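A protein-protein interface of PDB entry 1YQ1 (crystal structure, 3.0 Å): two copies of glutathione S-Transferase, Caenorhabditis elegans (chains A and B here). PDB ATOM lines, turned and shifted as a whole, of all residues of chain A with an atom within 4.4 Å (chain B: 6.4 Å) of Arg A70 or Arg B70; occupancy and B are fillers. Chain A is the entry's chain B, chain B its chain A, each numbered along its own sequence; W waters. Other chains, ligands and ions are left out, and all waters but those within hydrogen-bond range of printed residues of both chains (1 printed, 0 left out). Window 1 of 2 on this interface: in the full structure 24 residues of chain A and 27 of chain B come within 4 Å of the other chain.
NH2 of Arg A74 lies close to NH1 of Arg B74, at 3.0 Å.
The guanidinium group (NH1) of Arg B70 is in salt-bridge range of the side-chain carboxylate (OD2) of Asp A90.
NH1 of Arg A70 lies within salt-bridge range of OD2 of Asp B90, at 3.2 Å.
OE2 of Glu B86 is in salt-bridge range of NH1 of Arg A74, 3.1 Å away.
The guanidinium group (NH2) of Arg A70 sits close to the guanidinium group (NH1) of Arg B70 (3.1 Å).
The side-chain carboxylate of Asp B94 lies close to the backbone NH of Gly A66, at 3.5 Å.
OE1 of Glu B86 is in salt-bridge range of NE of Arg B74, 3.5 Å away.
The guanidinium group (NE) of Arg A70 is in salt-bridge range of the side-chain carboxylate (OD1) of Asp A90 (2.5 Å).
The side-chain carboxylate (OD1) of Asp B90 is in salt-bridge range of the guanidinium group (NE) of Arg B70, at 2.4 Å.
Printed residues of chain B that touch a printed residue of chain A: Arg B70, Arg B74, Glu B86, Asp B90, Ala B91 and Asp B94.
Hydrophobic or aromatic side chains of chain B within 4 Å of the printed part of chain A: Ala B91.
Of the 11 printed residues of chain A, 5 touch a printed residue of chain B.
Among the printed residues, Asp or Glu carboxylates within 4 Å of a Lys or Arg side-chain nitrogen of the other chain: Arg A70 with Asp B90 (3.2 Å), Arg A74 with Glu B86 (3.1 Å) and Asp A90 with Arg B70 (3.2 Å).
Of the printed residues of chain B, Ala A67 touches Ala B91 (3.6 Å) and Asp B94 (3.5 Å).
Of chain B, only Arg B70, Arg B74 and Asp B90 come within 4 Å of Arg A70.
Printed residues of chain B within 4 Å of Arg A74: Arg B74 (3.0 Å) and Glu B86 (3.1 Å).
Gly B66 touches none of the printed residues of chain A.
Of the printed residues of chain A, Arg B70 touches Arg A70 and Asp A90.
Printed residues of chain A within 4 Å of Glu B86: Arg A74.
Of the printed residues of chain A, Asp B90 touches Arg A70 (3.2 Å).
Of the printed residues of chain A, Asp B94 touches Gly A66 and Ala A67.
The nearest printed residue of chain A that does not touch Arg B70 is Gly A66 (6.9 Å).
The nearest printed residue of chain A that does not touch Asp B94 is Arg A70 (5.3 Å).
Among the printed residues, pairs that only touch across the chains: Ala A67 with Asp B94, Ala A67 with Ala B91 and Arg A70 with Arg B74.
Arg B70 touches its own counterpart, Arg A70.
Arg A70 touches Arg B74, but with the chains exchanged Arg A74 does not touch Arg B70 (7.1 Å).
Arg A70 touches Asp B90, and with the chains exchanged Asp A90 touches Arg B70.
Arg B74 touches its own counterpart, Arg A74.
Of the 9 pairs that touch across the chains among the printed residues, 4 have their exchanged pair printed and touching as well.
Water W1 bridges the guanidinium group of Arg B70 and the guanidinium group of Arg A70.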
ATOM      1  N   GLY A  66       7.161  20.103   3.452  1.00  0.00           N
ATOM      2  CA  GLY A  66       6.306  19.334   2.569  1.00  0.00           C
ATOM      3  C   GLY A  66       4.950  19.967   2.383  1.00  0.00           C
ATOM      4  O   GLY A  66       4.510  20.195   1.257  1.00  0.00           O
ATOM      5  N   ALA A  67       4.292  20.248   3.505  1.00  0.00           N
ATOM      6  CA  ALA A  67       2.969  20.860   3.508  1.00  0.00           C
ATOM      7  C   ALA A  67       3.011  22.212   2.827  1.00  0.00           C
ATOM      8  O   ALA A  67       2.156  22.534   1.998  1.00  0.00           O
ATOM      9  CB  ALA A  67       2.484  21.028   4.928  1.00  0.00           C
ATOM     10  N   ILE A  68       4.016  23.003   3.187  1.00  0.00           N
ATOM     11  CA  ILE A  68       4.172  24.332   2.629  1.00  0.00           C
ATOM     12  C   ILE A  68       4.367  24.248   1.130  1.00  0.00           C
ATOM     13  O   ILE A  68       3.673  24.919   0.371  1.00  0.00           O
ATOM     14  CB  ILE A  68       5.358  25.060   3.283  1.00  0.00           C
ATOM     15  CG1 ILE A  68       5.160  25.069   4.806  1.00  0.00           C
ATOM     16  CG2 ILE A  68       5.454  26.483   2.743  1.00  0.00           C
ATOM     17  CD1 ILE A  68       6.218  25.795   5.589  1.00  0.00           C
ATOM     18  N   LEU A  69       5.306  23.417   0.699  1.00  0.00           N
ATOM     19  CA  LEU A  69       5.547  23.261  -0.722  1.00  0.00           C
ATOM     20  C   LEU A  69       4.239  23.072  -1.475  1.00  0.00           C
ATOM     21  O   LEU A  69       3.924  23.826  -2.381  1.00  0.00           O
ATOM     22  CB  LEU A  69       6.451  22.060  -0.978  1.00  0.00           C
ATOM     23  CG  LEU A  69       7.929  22.330  -1.240  1.00  0.00           C
ATOM     24  CD1 LEU A  69       8.640  21.020  -1.560  1.00  0.00           C
ATOM     25  CD2 LEU A  69       8.061  23.299  -2.416  1.00  0.00           C
ATOM     26  N   ARG A  70       3.472  22.068  -1.078  1.00  0.00           N
ATOM     27  CA  ARG A  70       2.204  21.751  -1.728  1.00  0.00           C
ATOM     28  C   ARG A  70       1.160  22.862  -1.687  1.00  0.00           C
ATOM     29  O   ARG A  70       0.447  23.093  -2.669  1.00  0.00           O
ATOM     30  CB  ARG A  70       1.619  20.488  -1.099  1.00  0.00           C
ATOM     31  CG  ARG A  70       0.363  19.981  -1.764  1.00  0.00           C
ATOM     32  CD  ARG A  70      -0.047  18.621  -1.215  1.00  0.00           C
ATOM     33  NE  ARG A  70       1.053  17.666  -1.297  1.00  0.00           N
ATOM     34  CZ  ARG A  70       1.724  17.221  -0.244  1.00  0.00           C
ATOM     35  NH1 ARG A  70       1.387  17.627   0.969  1.00  0.00           N
ATOM     36  NH2 ARG A  70       2.719  16.358  -0.399  1.00  0.00           N
ATOM     37  N   TYR A  71       1.070  23.543  -0.546  1.00  0.00           N
ATOM     38  CA  TYR A  71       0.108  24.629  -0.354  1.00  0.00           C
ATOM     39  C   TYR A  71       0.276  25.726  -1.376  1.00  0.00           C
ATOM     40  O   TYR A  71      -0.694  26.218  -1.937  1.00  0.00           O
ATOM     41  CB  TYR A  71       0.275  25.243   1.023  1.00  0.00           C
ATOM     42  CG  TYR A  71      -0.753  26.290   1.326  1.00  0.00           C
ATOM     43  CD1 TYR A  71      -2.070  25.937   1.557  1.00  0.00           C
ATOM     44  CD2 TYR A  71      -0.401  27.635   1.431  1.00  0.00           C
ATOM     45  CE1 TYR A  71      -3.025  26.889   1.898  1.00  0.00           C
ATOM     46  CE2 TYR A  71      -1.354  28.607   1.775  1.00  0.00           C
ATOM     47  CZ  TYR A  71      -2.666  28.219   2.010  1.00  0.00           C
ATOM     48  OH  TYR A  71      -3.618  29.139   2.378  1.00  0.00           O
ATOM     49  N   LEU A  72       1.529  26.112  -1.586  1.00  0.00           N
ATOM     50  CA  LEU A  72       1.881  27.155  -2.531  1.00  0.00           C
ATOM     51  C   LEU A  72       1.804  26.609  -3.948  1.00  0.00           C
ATOM     52  O   LEU A  72       1.110  27.162  -4.795  1.00  0.00           O
ATOM     53  CB  LEU A  72       3.295  27.653  -2.228  1.00  0.00           C
ATOM     54  CG  LEU A  72       3.537  28.111  -0.787  1.00  0.00           C
ATOM     55  CD1 LEU A  72       5.019  28.356  -0.578  1.00  0.00           C
ATOM     56  CD2 LEU A  72       2.722  29.366  -0.490  1.00  0.00           C
ATOM     57  N   ALA A  73       2.516  25.517  -4.201  1.00  0.00           N
ATOM     58  CA  ALA A  73       2.510  24.899  -5.518  1.00  0.00           C
ATOM     59  C   ALA A  73       1.062  24.737  -5.982  1.00  0.00           C
ATOM     60  O   ALA A  73       0.748  24.865  -7.168  1.00  0.00           O
ATOM     61  CB  ALA A  73       3.192  23.552  -5.454  1.00  0.00           C
ATOM     62  N   ARG A  74       0.181  24.471  -5.023  1.00  0.00           N
ATOM     63  CA  ARG A  74      -1.237  24.289  -5.307  1.00  0.00           C
ATOM     64  C   ARG A  74      -1.882  25.588  -5.769  1.00  0.00           C
ATOM     65  O   ARG A  74      -2.600  25.622  -6.762  1.00  0.00           O
ATOM     66  CB  ARG A  74      -1.950  23.784  -4.063  1.00  0.00           C
ATOM     67  CG  ARG A  74      -3.156  22.953  -4.380  1.00  0.00           C
ATOM     68  CD  ARG A  74      -3.850  22.510  -3.110  1.00  0.00           C
ATOM     69  NE  ARG A  74      -4.959  21.610  -3.396  1.00  0.00           N
ATOM     70  CZ  ARG A  74      -5.750  21.092  -2.469  1.00  0.00           C
ATOM     71  NH1 ARG A  74      -5.552  21.392  -1.193  1.00  0.00           N
ATOM     72  NH2 ARG A  74      -6.729  20.271  -2.812  1.00  0.00           N
ATOM     73  N   ASP A  90       3.290  14.282  -5.491  1.00  0.00           N
ATOM     74  CA  ASP A  90       3.427  13.871  -4.096  1.00  0.00           C
ATOM     75  C   ASP A  90       4.235  12.572  -3.975  1.00  0.00           C
ATOM     76  O   ASP A  90       4.877  12.307  -2.956  1.00  0.00           O
ATOM     77  CB  ASP A  90       2.055  13.669  -3.444  1.00  0.00           C
ATOM     78  CG  ASP A  90       1.293  14.969  -3.256  1.00  0.00           C
ATOM     79  OD1 ASP A  90       1.928  16.003  -2.967  1.00  0.00           O
ATOM     80  OD2 ASP A  90       0.051  14.961  -3.380  1.00  0.00           O
ATOM     81  N   PHE A 157       6.702  21.222  -8.246  1.00  0.00           N
ATOM     82  CA  PHE A 157       7.588  21.283  -7.102  1.00  0.00           C
ATOM     83  C   PHE A 157       8.361  20.001  -6.882  1.00  0.00           C
ATOM     84  O   PHE A 157       9.123  19.897  -5.929  1.00  0.00           O
ATOM     85  CB  PHE A 157       6.819  21.707  -5.836  1.00  0.00           C
ATOM     86  CG  PHE A 157       5.981  20.627  -5.223  1.00  0.00           C
ATOM     87  CD1 PHE A 157       6.554  19.655  -4.409  1.00  0.00           C
ATOM     88  CD2 PHE A 157       4.608  20.595  -5.435  1.00  0.00           C
ATOM     89  CE1 PHE A 157       5.769  18.664  -3.814  1.00  0.00           C
ATOM     90  CE2 PHE A 157       3.813  19.612  -4.846  1.00  0.00           C
ATOM     91  CZ  PHE A 157       4.395  18.644  -4.032  1.00  0.00           C
ATOM     92  N   LEU B  21      -8.825   3.956   5.639  1.00  0.00           N
ATOM     93  CA  LEU B  21      -9.470   4.981   4.834  1.00  0.00           C
ATOM     94  C   LEU B  21     -10.564   4.420   3.931  1.00  0.00           C
ATOM     95  O   LEU B  21     -11.674   4.941   3.893  1.00  0.00           O
ATOM     96  CB  LEU B  21      -8.425   5.703   3.983  1.00  0.00           C
ATOM     97  CG  LEU B  21      -8.908   6.923   3.194  1.00  0.00           C
ATOM     98  CD1 LEU B  21      -9.433   7.997   4.152  1.00  0.00           C
ATOM     99  CD2 LEU B  21      -7.764   7.456   2.349  1.00  0.00           C
ATOM    100  N   SER B  65       2.778   5.642   0.224  1.00  0.00           N
ATOM    101  CA  SER B  65       1.799   5.596   1.303  1.00  0.00           C
ATOM    102  C   SER B  65       1.139   6.974   1.439  1.00  0.00           C
ATOM    103  O   SER B  65      -0.084   7.103   1.448  1.00  0.00           O
ATOM    104  CB  SER B  65       2.471   5.222   2.629  1.00  0.00           C
ATOM    105  OG  SER B  65       2.699   6.371   3.444  1.00  0.00           O
ATOM    106  N   GLY B  66       1.967   8.007   1.527  1.00  0.00           N
ATOM    107  CA  GLY B  66       1.458   9.355   1.668  1.00  0.00           C
ATOM    108  C   GLY B  66       0.752   9.868   0.432  1.00  0.00           C
ATOM    109  O   GLY B  66      -0.264  10.556   0.541  1.00  0.00           O
ATOM    110  N   ALA B  67       1.295   9.553  -0.742  1.00  0.00           N
ATOM    111  CA  ALA B  67       0.688   9.990  -1.991  1.00  0.00           C
ATOM    112  C   ALA B  67      -0.675   9.308  -2.093  1.00  0.00           C
ATOM    113  O   ALA B  67      -1.700   9.940  -2.360  1.00  0.00           O
ATOM    114  CB  ALA B  67       1.565   9.597  -3.155  1.00  0.00           C
ATOM    115  N   ILE B  68      -0.676   8.007  -1.845  1.00  0.00           N
ATOM    116  CA  ILE B  68      -1.880   7.209  -1.892  1.00  0.00           C
ATOM    117  C   ILE B  68      -2.903   7.726  -0.907  1.00  0.00           C
ATOM    118  O   ILE B  68      -4.058   7.884  -1.262  1.00  0.00           O
ATOM    119  CB  ILE B  68      -1.560   5.739  -1.597  1.00  0.00           C
ATOM    120  CG1 ILE B  68      -0.716   5.174  -2.737  1.00  0.00           C
ATOM    121  CG2 ILE B  68      -2.837   4.940  -1.454  1.00  0.00           C
ATOM    122  CD1 ILE B  68       0.057   3.955  -2.376  1.00  0.00           C
ATOM    123  N   LEU B  69      -2.505   7.997   0.328  1.00  0.00           N
ATOM    124  CA  LEU B  69      -3.475   8.517   1.293  1.00  0.00           C
ATOM    125  C   LEU B  69      -4.128   9.815   0.804  1.00  0.00           C
ATOM    126  O   LEU B  69      -5.337   9.862   0.573  1.00  0.00           O
ATOM    127  CB  LEU B  69      -2.815   8.773   2.648  1.00  0.00           C
ATOM    128  CG  LEU B  69      -2.498   7.564   3.521  1.00  0.00           C
ATOM    129  CD1 LEU B  69      -1.869   8.044   4.806  1.00  0.00           C
ATOM    130  CD2 LEU B  69      -3.771   6.794   3.817  1.00  0.00           C
ATOM    131  N   ARG B  70      -3.324  10.862   0.640  1.00  0.00           N
ATOM    132  CA  ARG B  70      -3.820  12.156   0.186  1.00  0.00           C
ATOM    133  C   ARG B  70      -4.658  12.016  -1.079  1.00  0.00           C
ATOM    134  O   ARG B  70      -5.721  12.623  -1.196  1.00  0.00           O
ATOM    135  CB  ARG B  70      -2.648  13.109  -0.079  1.00  0.00           C
ATOM    136  CG  ARG B  70      -3.040  14.574  -0.302  1.00  0.00           C
ATOM    137  CD  ARG B  70      -1.816  15.481  -0.283  1.00  0.00           C
ATOM    138  NE  ARG B  70      -0.976  15.208   0.881  1.00  0.00           N
ATOM    139  CZ  ARG B  70       0.175  14.545   0.836  1.00  0.00           C
ATOM    140  NH1 ARG B  70       0.651  14.116  -0.330  1.00  0.00           N
ATOM    141  NH2 ARG B  70       0.868  14.333   1.952  1.00  0.00           N
ATOM    142  N   TYR B  71      -4.184  11.219  -2.031  1.00  0.00           N
ATOM    143  CA  TYR B  71      -4.940  11.034  -3.261  1.00  0.00           C
ATOM    144  C   TYR B  71      -6.364  10.595  -2.971  1.00  0.00           C
ATOM    145  O   TYR B  71      -7.317  11.264  -3.347  1.00  0.00           O
ATOM    146  CB  TYR B  71      -4.307   9.979  -4.154  1.00  0.00           C
ATOM    147  CG  TYR B  71      -5.086   9.783  -5.426  1.00  0.00           C
ATOM    148  CD1 TYR B  71      -5.237  10.830  -6.322  1.00  0.00           C
ATOM    149  CD2 TYR B  71      -5.643   8.553  -5.753  1.00  0.00           C
ATOM    150  CE1 TYR B  71      -5.911  10.667  -7.519  1.00  0.00           C
ATOM    151  CE2 TYR B  71      -6.330   8.371  -6.963  1.00  0.00           C
ATOM    152  CZ  TYR B  71      -6.446   9.443  -7.839  1.00  0.00           C
ATOM    153  OH  TYR B  71      -7.032   9.305  -9.062  1.00  0.00           O
ATOM    154  N   LEU B  72      -6.488   9.449  -2.312  1.00  0.00           N
ATOM    155  CA  LEU B  72      -7.778   8.889  -1.978  1.00  0.00           C
ATOM    156  C   LEU B  72      -8.501   9.830  -1.052  1.00  0.00           C
ATOM    157  O   LEU B  72      -9.612  10.260  -1.348  1.00  0.00           O
ATOM    158  CB  LEU B  72      -7.609   7.537  -1.288  1.00  0.00           C
ATOM    159  CG  LEU B  72      -6.785   6.481  -2.028  1.00  0.00           C
ATOM    160  CD1 LEU B  72      -6.711   5.202  -1.178  1.00  0.00           C
ATOM    161  CD2 LEU B  72      -7.392   6.211  -3.399  1.00  0.00           C
ATOM    162  N   ALA B  73      -7.864  10.146   0.069  1.00  0.00           N
ATOM    163  CA  ALA B  73      -8.456  11.032   1.056  1.00  0.00           C
ATOM    164  C   ALA B  73      -9.125  12.246   0.400  1.00  0.00           C
ATOM    165  O   ALA B  73     -10.189  12.674   0.840  1.00  0.00           O
ATOM    166  CB  ALA B  73      -7.404  11.470   2.061  1.00  0.00           C
ATOM    167  N   ARG B  74      -8.515  12.807  -0.642  1.00  0.00           N
ATOM    168  CA  ARG B  74      -9.123  13.943  -1.339  1.00  0.00           C
ATOM    169  C   ARG B  74     -10.376  13.465  -2.059  1.00  0.00           C
ATOM    170  O   ARG B  74     -11.429  14.073  -1.915  1.00  0.00           O
ATOM    171  CB  ARG B  74      -8.158  14.578  -2.355  1.00  0.00           C
ATOM    172  CG  ARG B  74      -7.104  15.479  -1.721  1.00  0.00           C
ATOM    173  CD  ARG B  74      -6.480  16.453  -2.724  1.00  0.00           C
ATOM    174  NE  ARG B  74      -5.359  17.189  -2.129  1.00  0.00           N
ATOM    175  CZ  ARG B  74      -4.584  18.047  -2.789  1.00  0.00           C
ATOM    176  NH1 ARG B  74      -4.803  18.288  -4.071  1.00  0.00           N
ATOM    177  NH2 ARG B  74      -3.574  18.650  -2.175  1.00  0.00           N
ATOM    178  N   LYS B  75     -10.256  12.383  -2.833  1.00  0.00           N
ATOM    179  CA  LYS B  75     -11.378  11.799  -3.567  1.00  0.00           C
ATOM    180  C   LYS B  75     -12.483  11.351  -2.611  1.00  0.00           C
ATOM    181  O   LYS B  75     -13.671  11.511  -2.896  1.00  0.00           O
ATOM    182  CB  LYS B  75     -10.917  10.579  -4.376  1.00  0.00           C
ATOM    183  CG  LYS B  75     -10.579  10.853  -5.846  1.00  0.00           C
ATOM    184  CD  LYS B  75     -11.578  10.208  -6.830  1.00  0.00           C
ATOM    185  CE  LYS B  75     -11.340   8.721  -6.979  1.00  0.00           C
ATOM    186  NZ  LYS B  75      -9.982   8.419  -7.489  1.00  0.00           N
ATOM    187  N   ALA B  79      -9.476  14.650   3.591  1.00  0.00           N
ATOM    188  CA  ALA B  79      -8.163  15.262   3.455  1.00  0.00           C
ATOM    189  C   ALA B  79      -8.109  16.569   4.237  1.00  0.00           C
ATOM    190  O   ALA B  79      -7.033  17.110   4.490  1.00  0.00           O
ATOM    191  CB  ALA B  79      -7.865  15.524   1.971  1.00  0.00           C
ATOM    192  N   GLU B  86      -6.448  21.395   4.994  1.00  0.00           N
ATOM    193  CA  GLU B  86      -5.765  20.329   4.289  1.00  0.00           C
ATOM    194  C   GLU B  86      -4.253  20.422   4.482  1.00  0.00           C
ATOM    195  O   GLU B  86      -3.584  19.425   4.754  1.00  0.00           O
ATOM    196  CB  GLU B  86      -6.061  20.432   2.807  1.00  0.00           C
ATOM    197  CG  GLU B  86      -7.379  19.880   2.403  1.00  0.00           C
ATOM    198  CD  GLU B  86      -7.568  19.977   0.918  1.00  0.00           C
ATOM    199  OE1 GLU B  86      -7.134  19.040   0.207  1.00  0.00           O
ATOM    200  OE2 GLU B  86      -8.131  20.998   0.465  1.00  0.00           O
ATOM    201  N   VAL B  89      -3.310  19.038   7.656  1.00  0.00           N
ATOM    202  CA  VAL B  89      -3.380  17.583   7.687  1.00  0.00           C
ATOM    203  C   VAL B  89      -2.071  17.085   7.063  1.00  0.00           C
ATOM    204  O   VAL B  89      -1.424  16.183   7.596  1.00  0.00           O
ATOM    205  CB  VAL B  89      -4.583  17.043   6.871  1.00  0.00           C
ATOM    206  CG1 VAL B  89      -4.519  15.525   6.778  1.00  0.00           C
ATOM    207  CG2 VAL B  89      -5.885  17.450   7.536  1.00  0.00           C
ATOM    208  N   ASP B  90      -1.682  17.698   5.940  1.00  0.00           N
ATOM    209  CA  ASP B  90      -0.448  17.345   5.250  1.00  0.00           C
ATOM    210  C   ASP B  90       0.733  17.528   6.175  1.00  0.00           C
ATOM    211  O   ASP B  90       1.664  16.726   6.180  1.00  0.00           O
ATOM    212  CB  ASP B  90      -0.236  18.223   4.026  1.00  0.00           C
ATOM    213  CG  ASP B  90      -1.124  17.835   2.877  1.00  0.00           C
ATOM    214  OD1 ASP B  90      -1.466  16.643   2.787  1.00  0.00           O
ATOM    215  OD2 ASP B  90      -1.464  18.709   2.051  1.00  0.00           O
ATOM    216  N   ALA B  91       0.685  18.594   6.959  1.00  0.00           N
ATOM    217  CA  ALA B  91       1.759  18.901   7.890  1.00  0.00           C
ATOM    218  C   ALA B  91       1.811  17.925   9.041  1.00  0.00           C
ATOM    219  O   ALA B  91       2.877  17.471   9.409  1.00  0.00           O
ATOM    220  CB  ALA B  91       1.593  20.310   8.424  1.00  0.00           C
ATOM    221  N   HIS B  93       0.823  15.038   8.943  1.00  0.00           N
ATOM    222  CA  HIS B  93       1.275  13.783   8.330  1.00  0.00           C
ATOM    223  C   HIS B  93       2.806  13.735   8.212  1.00  0.00           C
ATOM    224  O   HIS B  93       3.434  12.731   8.543  1.00  0.00           O
ATOM    225  CB  HIS B  93       0.646  13.591   6.946  1.00  0.00           C
ATOM    226  CG  HIS B  93       1.050  12.313   6.275  1.00  0.00           C
ATOM    227  ND1 HIS B  93       2.184  12.205   5.499  1.00  0.00           N
ATOM    228  CD2 HIS B  93       0.488  11.081   6.291  1.00  0.00           C
ATOM    229  CE1 HIS B  93       2.300  10.964   5.062  1.00  0.00           C
ATOM    230  NE2 HIS B  93       1.285  10.261   5.530  1.00  0.00           N
ATOM    231  N   ASP B  94       3.393  14.822   7.732  1.00  0.00           N
ATOM    232  CA  ASP B  94       4.838  14.923   7.608  1.00  0.00           C
ATOM    233  C   ASP B  94       5.486  14.726   8.978  1.00  0.00           C
ATOM    234  O   ASP B  94       6.516  14.077   9.110  1.00  0.00           O
ATOM    235  CB  ASP B  94       5.221  16.306   7.076  1.00  0.00           C
ATOM    236  CG  ASP B  94       5.071  16.428   5.564  1.00  0.00           C
ATOM    237  OD1 ASP B  94       4.327  15.614   4.956  1.00  0.00           O
ATOM    238  OD2 ASP B  94       5.699  17.355   4.995  1.00  0.00           O
ATOM    239  N   PHE B 157      -7.464  11.899   7.250  1.00  0.00           N
ATOM    240  CA  PHE B 157      -6.542  10.786   7.040  1.00  0.00           C
ATOM    241  C   PHE B 157      -5.317  10.945   7.930  1.00  0.00           C
ATOM    242  O   PHE B 157      -4.558  10.001   8.110  1.00  0.00           O
ATOM    243  CB  PHE B 157      -6.138  10.652   5.555  1.00  0.00           C
ATOM    244  CG  PHE B 157      -5.049  11.592   5.105  1.00  0.00           C
ATOM    245  CD1 PHE B 157      -3.734  11.397   5.493  1.00  0.00           C
ATOM    246  CD2 PHE B 157      -5.338  12.640   4.234  1.00  0.00           C
ATOM    247  CE1 PHE B 157      -2.719  12.223   5.021  1.00  0.00           C
ATOM    248  CE2 PHE B 157      -4.328  13.474   3.754  1.00  0.00           C
ATOM    249  CZ  PHE B 157      -3.014  13.258   4.153  1.00  0.00           C
HETATM  250  O   HOH W   1       3.227  13.176   0.691  1.00  0.00           O
